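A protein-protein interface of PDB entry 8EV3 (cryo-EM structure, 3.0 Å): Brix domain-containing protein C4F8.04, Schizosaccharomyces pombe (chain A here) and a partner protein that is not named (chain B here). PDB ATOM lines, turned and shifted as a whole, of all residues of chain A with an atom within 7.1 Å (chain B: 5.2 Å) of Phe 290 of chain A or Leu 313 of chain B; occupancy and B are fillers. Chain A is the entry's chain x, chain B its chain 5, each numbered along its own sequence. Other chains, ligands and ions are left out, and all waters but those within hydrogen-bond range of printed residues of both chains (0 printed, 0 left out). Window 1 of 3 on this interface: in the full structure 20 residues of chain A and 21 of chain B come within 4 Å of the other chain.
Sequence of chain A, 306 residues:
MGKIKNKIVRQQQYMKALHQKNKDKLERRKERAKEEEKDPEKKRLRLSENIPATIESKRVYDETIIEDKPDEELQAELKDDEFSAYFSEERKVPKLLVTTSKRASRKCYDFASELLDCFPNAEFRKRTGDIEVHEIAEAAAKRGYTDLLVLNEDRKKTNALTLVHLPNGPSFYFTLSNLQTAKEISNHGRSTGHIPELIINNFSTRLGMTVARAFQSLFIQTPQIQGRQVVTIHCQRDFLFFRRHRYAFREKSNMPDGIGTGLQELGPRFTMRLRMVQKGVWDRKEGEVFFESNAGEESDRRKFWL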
ATOM      1  N   GLU A  77      -4.482  20.398  15.084  1.00  0.00           N
ATOM      2  CA  GLU A  77      -4.411  19.002  14.676  1.00  0.00           C
ATOM      3  C   GLU A  77      -4.904  18.792  13.250  1.00  0.00           C
ATOM      4  O   GLU A  77      -4.435  17.874  12.568  1.00  0.00           O
ATOM      5  CB  GLU A  77      -5.218  18.143  15.648  1.00  0.00           C
ATOM      6  CG  GLU A  77      -5.098  16.654  15.419  1.00  0.00           C
ATOM      7  CD  GLU A  77      -5.614  15.849  16.591  1.00  0.00           C
ATOM      8  OE1 GLU A  77      -6.019  16.463  17.600  1.00  0.00           O
ATOM      9  OE2 GLU A  77      -5.616  14.604  16.502  1.00  0.00           O
ATOM     10  N   PRO A 170      -6.888   7.622   6.523  1.00  0.00           N
ATOM     11  CA  PRO A 170      -7.773   6.689   7.223  1.00  0.00           C
ATOM     12  C   PRO A 170      -8.784   6.069   6.274  1.00  0.00           C
ATOM     13  O   PRO A 170      -9.230   6.693   5.310  1.00  0.00           O
ATOM     14  CB  PRO A 170      -8.460   7.568   8.274  1.00  0.00           C
ATOM     15  CG  PRO A 170      -7.655   8.819   8.340  1.00  0.00           C
ATOM     16  CD  PRO A 170      -7.056   9.004   6.991  1.00  0.00           C
ATOM     17  N   SER A 171      -9.142   4.824   6.561  1.00  0.00           N
ATOM     18  CA  SER A 171     -10.124   4.086   5.781  1.00  0.00           C
ATOM     19  C   SER A 171     -11.382   3.899   6.612  1.00  0.00           C
ATOM     20  O   SER A 171     -11.316   3.419   7.748  1.00  0.00           O
ATOM     21  CB  SER A 171      -9.568   2.731   5.348  1.00  0.00           C
ATOM     22  OG  SER A 171      -8.258   2.871   4.833  1.00  0.00           O
ATOM     23  N   PHE A 172     -12.520   4.282   6.047  1.00  0.00           N
ATOM     24  CA  PHE A 172     -13.808   4.192   6.717  1.00  0.00           C
ATOM     25  C   PHE A 172     -14.625   3.082   6.078  1.00  0.00           C
ATOM     26  O   PHE A 172     -14.724   3.010   4.850  1.00  0.00           O
ATOM     27  CB  PHE A 172     -14.566   5.519   6.632  1.00  0.00           C
ATOM     28  CG  PHE A 172     -13.788   6.697   7.140  1.00  0.00           C
ATOM     29  CD1 PHE A 172     -12.832   7.306   6.351  1.00  0.00           C
ATOM     30  CD2 PHE A 172     -14.023   7.202   8.402  1.00  0.00           C
ATOM     31  CE1 PHE A 172     -12.117   8.380   6.816  1.00  0.00           C
ATOM     32  CE2 PHE A 172     -13.312   8.280   8.869  1.00  0.00           C
ATOM     33  CZ  PHE A 172     -12.360   8.870   8.076  1.00  0.00           C
ATOM     34  N   ARG A 206     -16.203  14.488  18.133  1.00  0.00           N
ATOM     35  CA  ARG A 206     -14.876  14.563  17.530  1.00  0.00           C
ATOM     36  C   ARG A 206     -14.730  13.549  16.405  1.00  0.00           C
ATOM     37  O   ARG A 206     -14.157  13.856  15.353  1.00  0.00           O
ATOM     38  CB  ARG A 206     -13.804  14.341  18.595  1.00  0.00           C
ATOM     39  CG  ARG A 206     -12.387  14.339  18.055  1.00  0.00           C
ATOM     40  CD  ARG A 206     -11.924  15.739  17.719  1.00  0.00           C
ATOM     41  NE  ARG A 206     -10.655  15.735  17.003  1.00  0.00           N
ATOM     42  CZ  ARG A 206     -10.543  15.688  15.684  1.00  0.00           C
ATOM     43  NH1 ARG A 206     -11.607  15.635  14.903  1.00  0.00           N
ATOM     44  NH2 ARG A 206      -9.332  15.693  15.135  1.00  0.00           N
ATOM     45  N   LEU A 207     -15.239  12.334  16.609  1.00  0.00           N
ATOM     46  CA  LEU A 207     -15.247  11.343  15.539  1.00  0.00           C
ATOM     47  C   LEU A 207     -16.109  11.796  14.369  1.00  0.00           C
ATOM     48  O   LEU A 207     -15.881  11.376  13.230  1.00  0.00           O
ATOM     49  CB  LEU A 207     -15.734  10.002  16.082  1.00  0.00           C
ATOM     50  CG  LEU A 207     -15.617   8.773  15.187  1.00  0.00           C
ATOM     51  CD1 LEU A 207     -14.825   7.707  15.901  1.00  0.00           C
ATOM     52  CD2 LEU A 207     -16.991   8.253  14.831  1.00  0.00           C
ATOM     53  N   THR A 210     -13.886  13.811  11.857  1.00  0.00           N
ATOM     54  CA  THR A 210     -13.083  12.999  10.951  1.00  0.00           C
ATOM     55  C   THR A 210     -13.921  12.477   9.793  1.00  0.00           C
ATOM     56  O   THR A 210     -13.495  12.527   8.633  1.00  0.00           O
ATOM     57  CB  THR A 210     -12.446  11.839  11.713  1.00  0.00           C
ATOM     58  OG1 THR A 210     -11.638  12.354  12.776  1.00  0.00           O
ATOM     59  CG2 THR A 210     -11.580  11.013  10.787  1.00  0.00           C
ATOM     60  N   MET A 276     -16.549   0.803  11.119  1.00  0.00           N
ATOM     61  CA  MET A 276     -15.147   0.723  11.488  1.00  0.00           C
ATOM     62  C   MET A 276     -14.398   1.863  10.822  1.00  0.00           C
ATOM     63  O   MET A 276     -14.645   2.176   9.658  1.00  0.00           O
ATOM     64  CB  MET A 276     -14.547  -0.619  11.063  1.00  0.00           C
ATOM     65  CG  MET A 276     -13.045  -0.700  11.196  1.00  0.00           C
ATOM     66  SD  MET A 276     -12.537  -1.895  12.430  1.00  0.00           S
ATOM     67  CE  MET A 276     -12.594  -3.384  11.451  1.00  0.00           C
ATOM     68  N   VAL A 277     -13.491   2.478  11.571  1.00  0.00           N
ATOM     69  CA  VAL A 277     -12.544   3.446  11.039  1.00  0.00           C
ATOM     70  C   VAL A 277     -11.150   2.900  11.293  1.00  0.00           C
ATOM     71  O   VAL A 277     -10.808   2.565  12.431  1.00  0.00           O
ATOM     72  CB  VAL A 277     -12.714   4.835  11.681  1.00  0.00           C
ATOM     73  CG1 VAL A 277     -11.701   5.804  11.112  1.00  0.00           C
ATOM     74  CG2 VAL A 277     -14.118   5.349  11.463  1.00  0.00           C
ATOM     75  N   GLN A 278     -10.356   2.794  10.236  1.00  0.00           N
ATOM     76  CA  GLN A 278      -9.004   2.271  10.329  1.00  0.00           C
ATOM     77  C   GLN A 278      -8.004   3.376  10.037  1.00  0.00           C
ATOM     78  O   GLN A 278      -8.192   4.163   9.106  1.00  0.00           O
ATOM     79  CB  GLN A 278      -8.787   1.112   9.357  1.00  0.00           C
ATOM     80  CG  GLN A 278      -9.479  -0.170   9.750  1.00  0.00           C
ATOM     81  CD  GLN A 278      -8.761  -1.386   9.221  1.00  0.00           C
ATOM     82  OE1 GLN A 278      -8.172  -1.349   8.145  1.00  0.00           O
ATOM     83  NE2 GLN A 278      -8.809  -2.477   9.972  1.00  0.00           N
ATOM     84  N   LYS A 279      -6.950   3.439  10.840  1.00  0.00           N
ATOM     85  CA  LYS A 279      -5.836   4.336  10.566  1.00  0.00           C
ATOM     86  C   LYS A 279      -4.963   3.686   9.502  1.00  0.00           C
ATOM     87  O   LYS A 279      -4.371   2.627   9.735  1.00  0.00           O
ATOM     88  CB  LYS A 279      -5.047   4.615  11.840  1.00  0.00           C
ATOM     89  CG  LYS A 279      -4.055   5.752  11.716  1.00  0.00           C
ATOM     90  CD  LYS A 279      -3.031   5.707  12.836  1.00  0.00           C
ATOM     91  CE  LYS A 279      -2.004   4.615  12.601  1.00  0.00           C
ATOM     92  NZ  LYS A 279      -1.252   4.824  11.334  1.00  0.00           N
ATOM     93  N   GLY A 287      -5.329  -4.147  10.407  1.00  0.00           N
ATOM     94  CA  GLY A 287      -5.442  -2.702  10.408  1.00  0.00           C
ATOM     95  C   GLY A 287      -5.496  -2.150  11.818  1.00  0.00           C
ATOM     96  O   GLY A 287      -5.935  -2.829  12.748  1.00  0.00           O
ATOM     97  N   GLU A 288      -5.044  -0.907  11.973  1.00  0.00           N
ATOM     98  CA  GLU A 288      -5.104  -0.208  13.252  1.00  0.00           C
ATOM     99  C   GLU A 288      -6.509   0.350  13.425  1.00  0.00           C
ATOM    100  O   GLU A 288      -6.927   1.236  12.674  1.00  0.00           O
ATOM    101  CB  GLU A 288      -4.067   0.907  13.301  1.00  0.00           C
ATOM    102  CG  GLU A 288      -2.630   0.429  13.358  1.00  0.00           C
ATOM    103  CD  GLU A 288      -1.946   0.789  14.659  1.00  0.00           C
ATOM    104  OE1 GLU A 288      -2.655   1.093  15.638  1.00  0.00           O
ATOM    105  OE2 GLU A 288      -0.697   0.775  14.698  1.00  0.00           O
ATOM    106  N   VAL A 289      -7.238  -0.154  14.415  1.00  0.00           N
ATOM    107  CA  VAL A 289      -8.634   0.223  14.601  1.00  0.00           C
ATOM    108  C   VAL A 289      -8.684   1.594  15.263  1.00  0.00           C
ATOM    109  O   VAL A 289      -8.340   1.745  16.438  1.00  0.00           O
ATOM    110  CB  VAL A 289      -9.392  -0.824  15.424  1.00  0.00           C
ATOM    111  CG1 VAL A 289     -10.676  -0.246  15.975  1.00  0.00           C
ATOM    112  CG2 VAL A 289      -9.691  -2.023  14.564  1.00  0.00           C
ATOM    113  N   PHE A 290      -9.094   2.604  14.498  1.00  0.00           N
ATOM    114  CA  PHE A 290      -9.378   3.912  15.070  1.00  0.00           C
ATOM    115  C   PHE A 290     -10.703   3.910  15.816  1.00  0.00           C
ATOM    116  O   PHE A 290     -10.857   4.632  16.806  1.00  0.00           O
ATOM    117  CB  PHE A 290      -9.395   4.967  13.963  1.00  0.00           C
ATOM    118  CG  PHE A 290      -9.143   6.362  14.445  1.00  0.00           C
ATOM    119  CD1 PHE A 290     -10.145   7.090  15.054  1.00  0.00           C
ATOM    120  CD2 PHE A 290      -7.906   6.950  14.273  1.00  0.00           C
ATOM    121  CE1 PHE A 290      -9.915   8.374  15.493  1.00  0.00           C
ATOM    122  CE2 PHE A 290      -7.669   8.234  14.709  1.00  0.00           C
ATOM    123  CZ  PHE A 290      -8.675   8.947  15.320  1.00  0.00           C
ATOM    124  N   PHE A 291     -11.656   3.104  15.358  1.00  0.00           N
ATOM    125  CA  PHE A 291     -12.986   3.042  15.942  1.00  0.00           C
ATOM    126  C   PHE A 291     -13.653   1.767  15.452  1.00  0.00           C
ATOM    127  O   PHE A 291     -13.525   1.410  14.280  1.00  0.00           O
ATOM    128  CB  PHE A 291     -13.809   4.276  15.559  1.00  0.00           C
ATOM    129  CG  PHE A 291     -15.291   4.082  15.662  1.00  0.00           C
ATOM    130  CD1 PHE A 291     -15.932   4.181  16.882  1.00  0.00           C
ATOM    131  CD2 PHE A 291     -16.048   3.823  14.537  1.00  0.00           C
ATOM    132  CE1 PHE A 291     -17.295   4.011  16.978  1.00  0.00           C
ATOM    133  CE2 PHE A 291     -17.410   3.651  14.630  1.00  0.00           C
ATOM    134  CZ  PHE A 291     -18.032   3.747  15.852  1.00  0.00           C
ATOM    135  N   GLU A 292     -14.347   1.081  16.355  1.00  0.00           N
ATOM    136  CA  GLU A 292     -15.066  -0.141  16.015  1.00  0.00           C
ATOM    137  C   GLU A 292     -16.396  -0.133  16.746  1.00  0.00           C
ATOM    138  O   GLU A 292     -16.424  -0.173  17.979  1.00  0.00           O
ATOM    139  CB  GLU A 292     -14.255  -1.382  16.385  1.00  0.00           C
ATOM    140  CG  GLU A 292     -15.014  -2.682  16.227  1.00  0.00           C
ATOM    141  CD  GLU A 292     -14.690  -3.383  14.932  1.00  0.00           C
ATOM    142  OE1 GLU A 292     -13.558  -3.891  14.802  1.00  0.00           O
ATOM    143  OE2 GLU A 292     -15.566  -3.427  14.042  1.00  0.00           O
ATOM    144  N   LYS B 295     -11.052   1.255  24.010  1.00  0.00           N
ATOM    145  CA  LYS B 295     -11.440   1.337  22.612  1.00  0.00           C
ATOM    146  C   LYS B 295     -10.303   1.952  21.808  1.00  0.00           C
ATOM    147  O   LYS B 295      -9.475   2.690  22.344  1.00  0.00           O
ATOM    148  CB  LYS B 295     -12.712   2.169  22.439  1.00  0.00           C
ATOM    149  CG  LYS B 295     -13.759   1.944  23.515  1.00  0.00           C
ATOM    150  CD  LYS B 295     -14.610   0.726  23.209  1.00  0.00           C
ATOM    151  CE  LYS B 295     -15.924   0.768  23.962  1.00  0.00           C
ATOM    152  NZ  LYS B 295     -16.900   1.687  23.314  1.00  0.00           N
ATOM    153  N   GLY B 296     -10.249   1.620  20.522  1.00  0.00           N
ATOM    154  CA  GLY B 296      -9.199   2.139  19.666  1.00  0.00           C
ATOM    155  C   GLY B 296      -7.858   1.498  19.949  1.00  0.00           C
ATOM    156  O   GLY B 296      -7.555   1.167  21.098  1.00  0.00           O
ATOM    157  N   ALA B 297      -7.040   1.331  18.920  1.00  0.00           N
ATOM    158  CA  ALA B 297      -5.775   0.629  19.083  1.00  0.00           C
ATOM    159  C   ALA B 297      -4.894   1.369  20.083  1.00  0.00           C
ATOM    160  O   ALA B 297      -4.751   2.594  19.986  1.00  0.00           O
ATOM    161  CB  ALA B 297      -5.060   0.500  17.742  1.00  0.00           C
ATOM    162  N   PRO B 298      -4.287   0.675  21.048  1.00  0.00           N
ATOM    163  CA  PRO B 298      -3.501   1.368  22.076  1.00  0.00           C
ATOM    164  C   PRO B 298      -2.153   1.810  21.529  1.00  0.00           C
ATOM    165  O   PRO B 298      -1.395   1.006  20.983  1.00  0.00           O
ATOM    166  CB  PRO B 298      -3.340   0.314  23.178  1.00  0.00           C
ATOM    167  CG  PRO B 298      -3.601  -1.005  22.520  1.00  0.00           C
ATOM    168  CD  PRO B 298      -4.182  -0.788  21.153  1.00  0.00           C
ATOM    169  N   SER B 299      -1.861   3.104  21.670  1.00  0.00           N
ATOM    170  CA  SER B 299      -0.597   3.633  21.172  1.00  0.00           C
ATOM    171  C   SER B 299       0.567   3.235  22.070  1.00  0.00           C
ATOM    172  O   SER B 299       1.633   2.851  21.576  1.00  0.00           O
ATOM    173  CB  SER B 299      -0.679   5.151  21.047  1.00  0.00           C
ATOM    174  OG  SER B 299      -0.743   5.750  22.325  1.00  0.00           O
ATOM    175  N   THR B 311      -3.131   4.225  26.767  1.00  0.00           N
ATOM    176  CA  THR B 311      -3.587   5.313  25.917  1.00  0.00           C
ATOM    177  C   THR B 311      -3.522   4.857  24.466  1.00  0.00           C
ATOM    178  O   THR B 311      -2.673   4.044  24.094  1.00  0.00           O
ATOM    179  CB  THR B 311      -2.754   6.585  26.132  1.00  0.00           C
ATOM    180  OG1 THR B 311      -3.494   7.723  25.678  1.00  0.00           O
ATOM    181  CG2 THR B 311      -1.437   6.514  25.389  1.00  0.00           C
ATOM    182  N   GLY B 312      -4.439   5.354  23.657  1.00  0.00           N
ATOM    183  CA  GLY B 312      -4.563   4.882  22.292  1.00  0.00           C
ATOM    184  C   GLY B 312      -5.309   5.816  21.379  1.00  0.00           C
ATOM    185  O   GLY B 312      -5.301   7.034  21.565  1.00  0.00           O
ATOM    186  N   LEU B 313      -5.966   5.236  20.378  1.00  0.00           N
ATOM    187  CA  LEU B 313      -6.634   5.999  19.334  1.00  0.00           C
ATOM    188  C   LEU B 313      -8.025   6.475  19.729  1.00  0.00           C
ATOM    189  O   LEU B 313      -8.662   7.179  18.940  1.00  0.00           O
ATOM    190  CB  LEU B 313      -6.727   5.166  18.054  1.00  0.00           C
ATOM    191  CG  LEU B 313      -5.480   5.122  17.176  1.00  0.00           C
ATOM    192  CD1 LEU B 313      -5.733   4.273  15.950  1.00  0.00           C
ATOM    193  CD2 LEU B 313      -5.066   6.521  16.776  1.00  0.00           C
ATOM    194  N   ASP B 314      -8.514   6.115  20.909  1.00  0.00           N
ATOM    195  CA  ASP B 314      -9.774   6.661  21.392  1.00  0.00           C
ATOM    196  C   ASP B 314      -9.603   8.020  22.048  1.00  0.00           C
ATOM    197  O   ASP B 314     -10.567   8.542  22.617  1.00  0.00           O
ATOM    198  CB  ASP B 314     -10.441   5.690  22.370  1.00  0.00           C
ATOM    199  CG  ASP B 314      -9.564   5.363  23.561  1.00  0.00           C
ATOM    200  OD1 ASP B 314      -8.339   5.582  23.480  1.00  0.00           O
ATOM    201  OD2 ASP B 314     -10.099   4.877  24.578  1.00  0.00           O
ATOM    202  N   ARG B 315      -8.401   8.597  21.975  1.00  0.00           N
ATOM    203  CA  ARG B 315      -8.094   9.895  22.570  1.00  0.00           C
ATOM    204  C   ARG B 315      -8.390   9.907  24.064  1.00  0.00           C
ATOM    205  O   ARG B 315      -8.769  10.936  24.624  1.00  0.00           O
ATOM    206  CB  ARG B 315      -8.845  11.027  21.865  1.00  0.00           C
ATOM    207  CG  ARG B 315      -8.993  10.833  20.367  1.00  0.00           C
ATOM    208  CD  ARG B 315      -8.871  12.136  19.614  1.00  0.00           C
ATOM    209  NE  ARG B 315      -9.049  11.943  18.181  1.00  0.00           N
ATOM    210  CZ  ARG B 315      -8.274  12.484  17.251  1.00  0.00           C
ATOM    211  NH1 ARG B 315      -7.252  13.258  17.570  1.00  0.00           N
ATOM    212  NH2 ARG B 315      -8.532  12.240  15.969  1.00  0.00           N
ATOM    213  N   LEU B 335      -4.638  13.465  19.891  1.00  0.00           N
ATOM    214  CA  LEU B 335      -4.277  12.074  19.643  1.00  0.00           C
ATOM    215  C   LEU B 335      -2.954  11.753  20.323  1.00  0.00           C
ATOM    216  O   LEU B 335      -1.940  12.391  20.013  1.00  0.00           O
ATOM    217  CB  LEU B 335      -4.179  11.816  18.144  1.00  0.00           C
ATOM    218  CG  LEU B 335      -4.451  10.398  17.647  1.00  0.00           C
ATOM    219  CD1 LEU B 335      -5.845   9.952  18.036  1.00  0.00           C
ATOM    220  CD2 LEU B 335      -4.274  10.333  16.144  1.00  0.00           C
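Of chain B, only Leu 313 (3.7 Å) and Arg 315 (3.4 Å) come within 4 Å of Phe 290 of chain A. Of chain A, only Val 289 (3.7 Å) and Phe 290 (3.7 Å) come within 4 Å of Leu 313 of chain B. Of the printed residues of chain B, Arg 206 of chain A touches Arg 315. Printed residues of chain B within 4 Å of Glu 288 of chain A: Ala 297. Val 277 of chain A touches none of the printed residues of chain B. Ser 299 of chain B touches none of the printed residues of chain A. The nearest residue of chain B that does not touch Phe 290 of chain A is Leu 335 of chain B (4.05 Å). The nearest printed residue of chain A that does not touch Gly 296 of chain B is Phe 290 of chain A (4.1 Å).
The guanidinium group of Arg 315 of chain B lies within salt-bridge range of the side-chain carboxylate of Glu 77 of chain A, at 3.4 Å. The backbone carbonyl oxygen (O) of Val 289 of chain A sits at hydrogen-bond distance from the backbone NH (N) of Ala 297 of chain B (2.8 Å).
Of the 11 printed residues of chain B, 5 touch a printed residue of chain A. Hydrophobic or aromatic side chains of chain B within 4 Å of the printed part of chain A: Ala 297, Leu 313 and Leu 335. Printed residues of chain A that touch a printed residue of chain B: Glu 77, Arg 206, Glu 288, Val 289 and Phe 290. Hydrophobic or aromatic side chains of chain A that line the printed part of chain B: Phe 290.
Among the printed residues, pairs that only touch across the chains: Glu 77 of chain A with Leu 335 of chain B (3.5 Å), Arg 206 of chain A with Arg 315 of chain B (3.6 Å), Glu 288 of chain A with Ala 297 of chain B (3.2 Å), Val 289 of chain A with Gly 296 of chain B (3.4 Å), Val 289 of chain A with Leu 313 of chain B (3.7 Å), Phe 290 of chain A with Leu 313 of chain B (3.7 Å) and Phe 290 of chain A with Arg 315 of chain B (3.4 Å).
The backbone NH of Phe 290 of chain A is in hydrogen-bond range of the backbone carbonyl oxygen of Val 277 of chain A (2.7 Å). The backbone carbonyl oxygen of Glu 288 of chain A lies within hydrogen-bond range of the backbone NH of Lys 279 of chain A. The backbone NH of Leu 313 of chain B lies within hydrogen-bond range of the backbone carbonyl oxygen of Ala 297 of chain B (2.9 Å).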
